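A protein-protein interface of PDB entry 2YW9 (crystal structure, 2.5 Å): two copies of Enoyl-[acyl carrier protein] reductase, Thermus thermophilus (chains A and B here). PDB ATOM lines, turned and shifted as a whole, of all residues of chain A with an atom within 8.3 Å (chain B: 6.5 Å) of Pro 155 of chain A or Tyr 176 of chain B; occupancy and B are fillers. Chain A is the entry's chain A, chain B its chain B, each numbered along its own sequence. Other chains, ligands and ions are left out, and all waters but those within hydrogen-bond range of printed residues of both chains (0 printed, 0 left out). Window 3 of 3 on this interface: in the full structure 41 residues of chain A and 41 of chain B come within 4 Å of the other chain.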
ATOM      1  N   MET A 102      -0.438 -36.693  -9.071  1.00  0.00           N
ATOM      2  CA  MET A 102      -0.357 -35.295  -8.639  1.00  0.00           C
ATOM      3  C   MET A 102       0.892 -34.996  -7.803  1.00  0.00           C
ATOM      4  O   MET A 102       1.232 -33.838  -7.565  1.00  0.00           O
ATOM      5  CB  MET A 102      -1.631 -34.890  -7.890  1.00  0.00           C
ATOM      6  CG  MET A 102      -2.893 -34.992  -8.745  1.00  0.00           C
ATOM      7  SD  MET A 102      -2.830 -33.969 -10.238  1.00  0.00           S
ATOM      8  CE  MET A 102      -3.086 -32.345  -9.534  1.00  0.00           C
ATOM      9  N   GLY A 104       4.882 -35.138  -7.748  1.00  0.00           N
ATOM     10  CA  GLY A 104       6.021 -35.226  -8.650  1.00  0.00           C
ATOM     11  C   GLY A 104       5.789 -34.555  -9.993  1.00  0.00           C
ATOM     12  O   GLY A 104       4.945 -33.663 -10.120  1.00  0.00           O
ATOM     13  N   ARG A 105       6.542 -34.986 -11.000  1.00  0.00           N
ATOM     14  CA  ARG A 105       6.491 -34.360 -12.318  1.00  0.00           C
ATOM     15  C   ARG A 105       5.457 -35.000 -13.222  1.00  0.00           C
ATOM     16  O   ARG A 105       5.181 -36.192 -13.113  1.00  0.00           O
ATOM     17  CB  ARG A 105       7.846 -34.452 -13.004  1.00  0.00           C
ATOM     18  CG  ARG A 105       9.010 -34.033 -12.147  1.00  0.00           C
ATOM     19  CD  ARG A 105      10.206 -34.918 -12.453  1.00  0.00           C
ATOM     20  NE  ARG A 105      11.064 -34.365 -13.493  1.00  0.00           N
ATOM     21  CZ  ARG A 105      11.746 -35.097 -14.370  1.00  0.00           C
ATOM     22  NH1 ARG A 105      11.653 -36.426 -14.372  1.00  0.00           N
ATOM     23  NH2 ARG A 105      12.507 -34.495 -15.266  1.00  0.00           N
ATOM     24  N   TYR A 106       4.905 -34.196 -14.127  1.00  0.00           N
ATOM     25  CA  TYR A 106       3.947 -34.682 -15.121  1.00  0.00           C
ATOM     26  C   TYR A 106       4.546 -35.788 -15.985  1.00  0.00           C
ATOM     27  O   TYR A 106       3.882 -36.768 -16.316  1.00  0.00           O
ATOM     28  CB  TYR A 106       3.464 -33.537 -16.014  1.00  0.00           C
ATOM     29  CG  TYR A 106       2.592 -34.018 -17.148  1.00  0.00           C
ATOM     30  CD1 TYR A 106       2.973 -33.842 -18.479  1.00  0.00           C
ATOM     31  CD2 TYR A 106       1.394 -34.683 -16.887  1.00  0.00           C
ATOM     32  CE1 TYR A 106       2.171 -34.298 -19.522  1.00  0.00           C
ATOM     33  CE2 TYR A 106       0.592 -35.142 -17.914  1.00  0.00           C
ATOM     34  CZ  TYR A 106       0.981 -34.950 -19.228  1.00  0.00           C
ATOM     35  OH  TYR A 106       0.164 -35.410 -20.230  1.00  0.00           O
ATOM     36  N   TYR A 147      -9.884 -25.034 -15.240  1.00  0.00           N
ATOM     37  CA  TYR A 147      -8.893 -24.165 -14.633  1.00  0.00           C
ATOM     38  C   TYR A 147      -7.879 -23.733 -15.683  1.00  0.00           C
ATOM     39  O   TYR A 147      -7.662 -24.421 -16.686  1.00  0.00           O
ATOM     40  CB  TYR A 147      -8.208 -24.883 -13.465  1.00  0.00           C
ATOM     41  CG  TYR A 147      -7.152 -24.068 -12.755  1.00  0.00           C
ATOM     42  CD1 TYR A 147      -7.500 -23.032 -11.895  1.00  0.00           C
ATOM     43  CD2 TYR A 147      -5.801 -24.340 -12.935  1.00  0.00           C
ATOM     44  CE1 TYR A 147      -6.520 -22.280 -11.234  1.00  0.00           C
ATOM     45  CE2 TYR A 147      -4.818 -23.598 -12.287  1.00  0.00           C
ATOM     46  CZ  TYR A 147      -5.184 -22.575 -11.435  1.00  0.00           C
ATOM     47  OH  TYR A 147      -4.208 -21.845 -10.791  1.00  0.00           O
ATOM     48  N   ALA A 149      -4.745 -23.713 -15.867  1.00  0.00           N
ATOM     49  CA  ALA A 149      -3.621 -24.611 -16.119  1.00  0.00           C
ATOM     50  C   ALA A 149      -3.751 -25.370 -17.444  1.00  0.00           C
ATOM     51  O   ALA A 149      -2.769 -25.901 -17.962  1.00  0.00           O
ATOM     52  CB  ALA A 149      -3.458 -25.588 -14.971  1.00  0.00           C
ATOM     53  N   LYS A 152      -1.995 -22.553 -19.672  1.00  0.00           N
ATOM     54  CA  LYS A 152      -0.664 -22.145 -19.233  1.00  0.00           C
ATOM     55  C   LYS A 152      -0.123 -23.126 -18.209  1.00  0.00           C
ATOM     56  O   LYS A 152      -0.888 -23.739 -17.469  1.00  0.00           O
ATOM     57  CB  LYS A 152      -0.700 -20.735 -18.638  1.00  0.00           C
ATOM     58  CG  LYS A 152      -1.151 -19.639 -19.597  1.00  0.00           C
ATOM     59  CD  LYS A 152      -0.144 -19.385 -20.710  1.00  0.00           C
ATOM     60  CE  LYS A 152      -0.679 -18.350 -21.681  1.00  0.00           C
ATOM     61  NZ  LYS A 152       0.247 -18.142 -22.829  1.00  0.00           N
ATOM     62  N   VAL A 153       1.197 -23.283 -18.167  1.00  0.00           N
ATOM     63  CA  VAL A 153       1.800 -24.239 -17.243  1.00  0.00           C
ATOM     64  C   VAL A 153       1.705 -23.746 -15.805  1.00  0.00           C
ATOM     65  O   VAL A 153       2.295 -22.726 -15.434  1.00  0.00           O
ATOM     66  CB  VAL A 153       3.267 -24.571 -17.594  1.00  0.00           C
ATOM     67  CG1 VAL A 153       3.834 -25.581 -16.605  1.00  0.00           C
ATOM     68  CG2 VAL A 153       3.366 -25.117 -18.998  1.00  0.00           C
ATOM     69  N   VAL A 154       0.921 -24.467 -15.015  1.00  0.00           N
ATOM     70  CA  VAL A 154       0.886 -24.261 -13.583  1.00  0.00           C
ATOM     71  C   VAL A 154       1.475 -25.524 -12.975  1.00  0.00           C
ATOM     72  O   VAL A 154       0.857 -26.590 -13.027  1.00  0.00           O
ATOM     73  CB  VAL A 154      -0.550 -24.029 -13.066  1.00  0.00           C
ATOM     74  CG1 VAL A 154      -0.548 -23.837 -11.550  1.00  0.00           C
ATOM     75  CG2 VAL A 154      -1.177 -22.820 -13.758  1.00  0.00           C
ATOM     76  N   PRO A 155       2.696 -25.414 -12.430  1.00  0.00           N
ATOM     77  CA  PRO A 155       3.425 -26.557 -11.877  1.00  0.00           C
ATOM     78  C   PRO A 155       2.660 -27.215 -10.734  1.00  0.00           C
ATOM     79  O   PRO A 155       1.973 -26.529  -9.971  1.00  0.00           O
ATOM     80  CB  PRO A 155       4.724 -25.929 -11.360  1.00  0.00           C
ATOM     81  CG  PRO A 155       4.861 -24.644 -12.133  1.00  0.00           C
ATOM     82  CD  PRO A 155       3.458 -24.161 -12.318  1.00  0.00           C
ATOM     83  N   LYS A 156       2.773 -28.535 -10.643  1.00  0.00           N
ATOM     84  CA  LYS A 156       2.093 -29.333  -9.614  1.00  0.00           C
ATOM     85  C   LYS A 156       0.624 -29.589  -9.949  1.00  0.00           C
ATOM     86  O   LYS A 156      -0.081 -30.271  -9.202  1.00  0.00           O
ATOM     87  CB  LYS A 156       2.242 -28.719  -8.209  1.00  0.00           C
ATOM     88  N   TYR A 157       0.164 -29.053 -11.074  1.00  0.00           N
ATOM     89  CA  TYR A 157      -1.173 -29.374 -11.551  1.00  0.00           C
ATOM     90  C   TYR A 157      -1.147 -30.637 -12.407  1.00  0.00           C
ATOM     91  O   TYR A 157      -2.165 -31.318 -12.566  1.00  0.00           O
ATOM     92  CB  TYR A 157      -1.744 -28.222 -12.358  1.00  0.00           C
ATOM     93  CG  TYR A 157      -3.041 -27.731 -11.794  1.00  0.00           C
ATOM     94  CD1 TYR A 157      -3.060 -26.657 -10.908  1.00  0.00           C
ATOM     95  CD2 TYR A 157      -4.247 -28.355 -12.109  1.00  0.00           C
ATOM     96  CE1 TYR A 157      -4.241 -26.202 -10.361  1.00  0.00           C
ATOM     97  CE2 TYR A 157      -5.445 -27.907 -11.568  1.00  0.00           C
ATOM     98  CZ  TYR A 157      -5.433 -26.826 -10.694  1.00  0.00           C
ATOM     99  OH  TYR A 157      -6.615 -26.357 -10.146  1.00  0.00           O
ATOM    100  N   ASN A 158       0.030 -30.925 -12.959  1.00  0.00           N
ATOM    101  CA  ASN A 158       0.283 -32.133 -13.732  1.00  0.00           C
ATOM    102  C   ASN A 158      -0.867 -32.535 -14.655  1.00  0.00           C
ATOM    103  O   ASN A 158      -1.362 -31.718 -15.430  1.00  0.00           O
ATOM    104  CB  ASN A 158       0.665 -33.286 -12.802  1.00  0.00           C
ATOM    105  CG  ASN A 158       1.960 -33.022 -12.037  1.00  0.00           C
ATOM    106  OD1 ASN A 158       2.684 -32.067 -12.326  1.00  0.00           O
ATOM    107  ND2 ASN A 158       2.256 -33.875 -11.060  1.00  0.00           N
ATOM    108  N   ALA A 161      -4.208 -30.613 -15.596  1.00  0.00           N
ATOM    109  CA  ALA A 161      -4.128 -29.570 -16.614  1.00  0.00           C
ATOM    110  C   ALA A 161      -4.439 -30.134 -17.990  1.00  0.00           C
ATOM    111  O   ALA A 161      -5.113 -29.501 -18.803  1.00  0.00           O
ATOM    112  CB  ALA A 161      -2.754 -28.962 -16.617  1.00  0.00           C
ATOM    113  N   VAL B 171       2.852 -30.933 -24.335  1.00  0.00           N
ATOM    114  CA  VAL B 171       4.032 -30.296 -24.891  1.00  0.00           C
ATOM    115  C   VAL B 171       4.473 -29.137 -24.014  1.00  0.00           C
ATOM    116  O   VAL B 171       5.667 -28.978 -23.758  1.00  0.00           O
ATOM    117  CB  VAL B 171       3.792 -29.823 -26.345  1.00  0.00           C
ATOM    118  CG1 VAL B 171       4.798 -28.763 -26.760  1.00  0.00           C
ATOM    119  CG2 VAL B 171       3.853 -31.001 -27.279  1.00  0.00           C
ATOM    120  N   ARG B 172       3.514 -28.342 -23.544  1.00  0.00           N
ATOM    121  CA  ARG B 172       3.835 -27.203 -22.681  1.00  0.00           C
ATOM    122  C   ARG B 172       4.483 -27.640 -21.359  1.00  0.00           C
ATOM    123  O   ARG B 172       5.554 -27.158 -20.994  1.00  0.00           O
ATOM    124  CB  ARG B 172       2.595 -26.336 -22.429  1.00  0.00           C
ATOM    125  CG  ARG B 172       2.197 -25.515 -23.635  1.00  0.00           C
ATOM    126  CD  ARG B 172       1.102 -24.517 -23.319  1.00  0.00           C
ATOM    127  NE  ARG B 172      -0.200 -25.158 -23.144  1.00  0.00           N
ATOM    128  CZ  ARG B 172      -0.997 -25.536 -24.142  1.00  0.00           C
ATOM    129  NH1 ARG B 172      -0.628 -25.357 -25.406  1.00  0.00           N
ATOM    130  NH2 ARG B 172      -2.166 -26.102 -23.875  1.00  0.00           N
ATOM    131  N   TYR B 173       3.832 -28.569 -20.669  1.00  0.00           N
ATOM    132  CA  TYR B 173       4.327 -29.082 -19.409  1.00  0.00           C
ATOM    133  C   TYR B 173       5.661 -29.816 -19.561  1.00  0.00           C
ATOM    134  O   TYR B 173       6.544 -29.692 -18.704  1.00  0.00           O
ATOM    135  CB  TYR B 173       3.273 -29.964 -18.735  1.00  0.00           C
ATOM    136  CG  TYR B 173       2.284 -29.166 -17.912  1.00  0.00           C
ATOM    137  CD1 TYR B 173       1.291 -28.408 -18.524  1.00  0.00           C
ATOM    138  CD2 TYR B 173       2.357 -29.156 -16.520  1.00  0.00           C
ATOM    139  CE1 TYR B 173       0.400 -27.670 -17.781  1.00  0.00           C
ATOM    140  CE2 TYR B 173       1.463 -28.427 -15.765  1.00  0.00           C
ATOM    141  CZ  TYR B 173       0.488 -27.685 -16.400  1.00  0.00           C
ATOM    142  OH  TYR B 173      -0.399 -26.949 -15.652  1.00  0.00           O
ATOM    143  N   LEU B 174       5.815 -30.563 -20.652  1.00  0.00           N
ATOM    144  CA  LEU B 174       7.079 -31.242 -20.920  1.00  0.00           C
ATOM    145  C   LEU B 174       8.210 -30.260 -21.227  1.00  0.00           C
ATOM    146  O   LEU B 174       9.364 -30.514 -20.884  1.00  0.00           O
ATOM    147  CB  LEU B 174       6.932 -32.247 -22.055  1.00  0.00           C
ATOM    148  CG  LEU B 174       6.085 -33.479 -21.748  1.00  0.00           C
ATOM    149  CD1 LEU B 174       5.959 -34.345 -22.991  1.00  0.00           C
ATOM    150  CD2 LEU B 174       6.679 -34.269 -20.601  1.00  0.00           C
ATOM    151  N   ALA B 175       7.877 -29.142 -21.864  1.00  0.00           N
ATOM    152  CA  ALA B 175       8.863 -28.114 -22.177  1.00  0.00           C
ATOM    153  C   ALA B 175       9.377 -27.474 -20.906  1.00  0.00           C
ATOM    154  O   ALA B 175      10.542 -27.100 -20.823  1.00  0.00           O
ATOM    155  CB  ALA B 175       8.269 -27.053 -23.084  1.00  0.00           C
ATOM    156  N   TYR B 176       8.491 -27.337 -19.926  1.00  0.00           N
ATOM    157  CA  TYR B 176       8.852 -26.754 -18.647  1.00  0.00           C
ATOM    158  C   TYR B 176       9.719 -27.720 -17.843  1.00  0.00           C
ATOM    159  O   TYR B 176      10.719 -27.320 -17.245  1.00  0.00           O
ATOM    160  CB  TYR B 176       7.596 -26.356 -17.869  1.00  0.00           C
ATOM    161  CG  TYR B 176       7.794 -26.260 -16.379  1.00  0.00           C
ATOM    162  CD1 TYR B 176       8.550 -25.235 -15.819  1.00  0.00           C
ATOM    163  CD2 TYR B 176       7.214 -27.195 -15.525  1.00  0.00           C
ATOM    164  CE1 TYR B 176       8.732 -25.149 -14.444  1.00  0.00           C
ATOM    165  CE2 TYR B 176       7.392 -27.122 -14.153  1.00  0.00           C
ATOM    166  CZ  TYR B 176       8.151 -26.098 -13.622  1.00  0.00           C
ATOM    167  OH  TYR B 176       8.318 -26.029 -12.264  1.00  0.00           O
ATOM    168  N   GLU B 177       9.347 -28.992 -17.846  1.00  0.00           N
ATOM    169  CA  GLU B 177      10.059 -29.981 -17.045  1.00  0.00           C
ATOM    170  C   GLU B 177      11.405 -30.414 -17.653  1.00  0.00           C
ATOM    171  O   GLU B 177      12.366 -30.620 -16.921  1.00  0.00           O
ATOM    172  CB  GLU B 177       9.155 -31.179 -16.730  1.00  0.00           C
ATOM    173  CG  GLU B 177       7.968 -30.818 -15.842  1.00  0.00           C
ATOM    174  CD  GLU B 177       7.036 -31.986 -15.570  1.00  0.00           C
ATOM    175  OE1 GLU B 177       6.176 -31.872 -14.671  1.00  0.00           O
ATOM    176  OE2 GLU B 177       7.146 -33.019 -16.258  1.00  0.00           O
ATOM    177  N   LEU B 178      11.484 -30.517 -18.979  1.00  0.00           N
ATOM    178  CA  LEU B 178      12.732 -30.924 -19.647  1.00  0.00           C
ATOM    179  C   LEU B 178      13.640 -29.759 -20.038  1.00  0.00           C
ATOM    180  O   LEU B 178      14.767 -29.968 -20.495  1.00  0.00           O
ATOM    181  CB  LEU B 178      12.438 -31.761 -20.890  1.00  0.00           C
ATOM    182  CG  LEU B 178      11.585 -33.014 -20.701  1.00  0.00           C
ATOM    183  CD1 LEU B 178      11.395 -33.706 -22.028  1.00  0.00           C
ATOM    184  CD2 LEU B 178      12.206 -33.949 -19.689  1.00  0.00           C
ATOM    185  N   GLY B 179      13.148 -28.538 -19.867  1.00  0.00           N
ATOM    186  CA  GLY B 179      13.905 -27.342 -20.234  1.00  0.00           C
ATOM    187  C   GLY B 179      15.242 -27.138 -19.531  1.00  0.00           C
ATOM    188  O   GLY B 179      16.241 -26.838 -20.188  1.00  0.00           O
ATOM    189  N   PRO B 180      15.274 -27.280 -18.190  1.00  0.00           N
ATOM    190  CA  PRO B 180      16.508 -27.030 -17.430  1.00  0.00           C
ATOM    191  C   PRO B 180      17.695 -27.872 -17.893  1.00  0.00           C
ATOM    192  O   PRO B 180      18.841 -27.425 -17.791  1.00  0.00           O
ATOM    193  CB  PRO B 180      16.123 -27.406 -15.993  1.00  0.00           C
ATOM    194  CG  PRO B 180      14.651 -27.209 -15.944  1.00  0.00           C
ATOM    195  CD  PRO B 180      14.156 -27.641 -17.300  1.00  0.00           C
ATOM    196  N   VAL B 185      10.846 -28.827 -26.298  1.00  0.00           N
ATOM    197  CA  VAL B 185       9.694 -29.603 -26.732  1.00  0.00           C
ATOM    198  C   VAL B 185       8.743 -28.684 -27.487  1.00  0.00           C
ATOM    199  O   VAL B 185       8.393 -27.614 -27.002  1.00  0.00           O
ATOM    200  CB  VAL B 185       8.971 -30.247 -25.540  1.00  0.00           C
ATOM    201  CG1 VAL B 185       7.974 -31.287 -26.012  1.00  0.00           C
ATOM    202  CG2 VAL B 185       9.977 -30.882 -24.591  1.00  0.00           C
ATOM    203  N   THR B 242      10.729 -23.062 -27.559  1.00  0.00           N
ATOM    204  CA  THR B 242      10.230 -24.234 -26.832  1.00  0.00           C
ATOM    205  C   THR B 242       8.814 -24.028 -26.285  1.00  0.00           C
ATOM    206  O   THR B 242       8.388 -22.906 -26.033  1.00  0.00           O
ATOM    207  CB  THR B 242      11.181 -24.680 -25.694  1.00  0.00           C
ATOM    208  OG1 THR B 242      10.798 -25.981 -25.231  1.00  0.00           O
ATOM    209  CG2 THR B 242      11.145 -23.697 -24.529  1.00  0.00           C
ATOM    210  N   GLY B 243       8.084 -25.124 -26.121  1.00  0.00           N
ATOM    211  CA  GLY B 243       6.700 -25.073 -25.659  1.00  0.00           C
ATOM    212  C   GLY B 243       5.733 -24.541 -26.700  1.00  0.00           C
ATOM    213  O   GLY B 243       4.578 -24.260 -26.389  1.00  0.00           O
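Of the 13 printed residues of chain B, 4 touch a printed residue of chain A. Hydrophobic or aromatic side chains of chain B within 4 Å of the printed part of chain A: Tyr 173 and Tyr 176. Hydrophobic or aromatic side chains of chain A within 4 Å of the printed part of chain B: Tyr 106, Ala 149, Val 153, Val 154, Pro 155, Tyr 157 and Ala 161. Among the printed residues, no Asp or Glu carboxylate lies within 4 Å of a Lys or Arg side-chain nitrogen of the other chain.
Printed residues of chain B within 4 Å of Arg 105 of chain A: Glu 177 (3.4 Å). Printed residues of chain B within 4 Å of Tyr 106 of chain A: Tyr 173 and Glu 177. Of the printed residues of chain B, Lys 152 of chain A touches Tyr 173. Pro 155 of chain A touches just one residue of chain B: Tyr 176 (3.7 Å). Of the printed residues of chain A, Arg 172 of chain B touches Val 153 (3.6 Å). No residue of chain A comes within 4 Å of Ala 175 of chain B. Of chain A, only Val 153 and Pro 155 come within 4 Å of Tyr 176 of chain B. Of the printed residues of chain A, Glu 177 of chain B touches Arg 105 and Tyr 106.
N of Tyr 106 of chain A is in hydrogen-bond range of OE1 of Glu 177 of chain B, at 2.7 Å. OH of Tyr 173 of chain B sits close to O of Ala 149 of chain A (3.5 Å). The backbone NH (N) of Val 154 of chain A sits at hydrogen-bond distance from the side-chain hydroxyl (OH) of Tyr 173 of chain B, 2.9 Å away.
No position is printed for both chains. Of the 12 pairs that touch across the chains among the printed residues, none has its exchanged pair printed and touching as well.
Among the printed residues, merely in contact across the chains: Ala 161 of chain A with Tyr 173 of chain B, Arg 105 of chain A with Glu 177 of chain B, Val 153 of chain A with Arg 172 of chain B, Pro 155 of chain A with Tyr 176 of chain B, Lys 152 of chain A with Tyr 173 of chain B, Val 153 of chain A with Tyr 173 of chain B, Tyr 157 of chain A with Tyr 173 of chain B, Tyr 106 of chain A with Tyr 173 of chain B and Val 153 of chain A with Tyr 176 of chain B.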
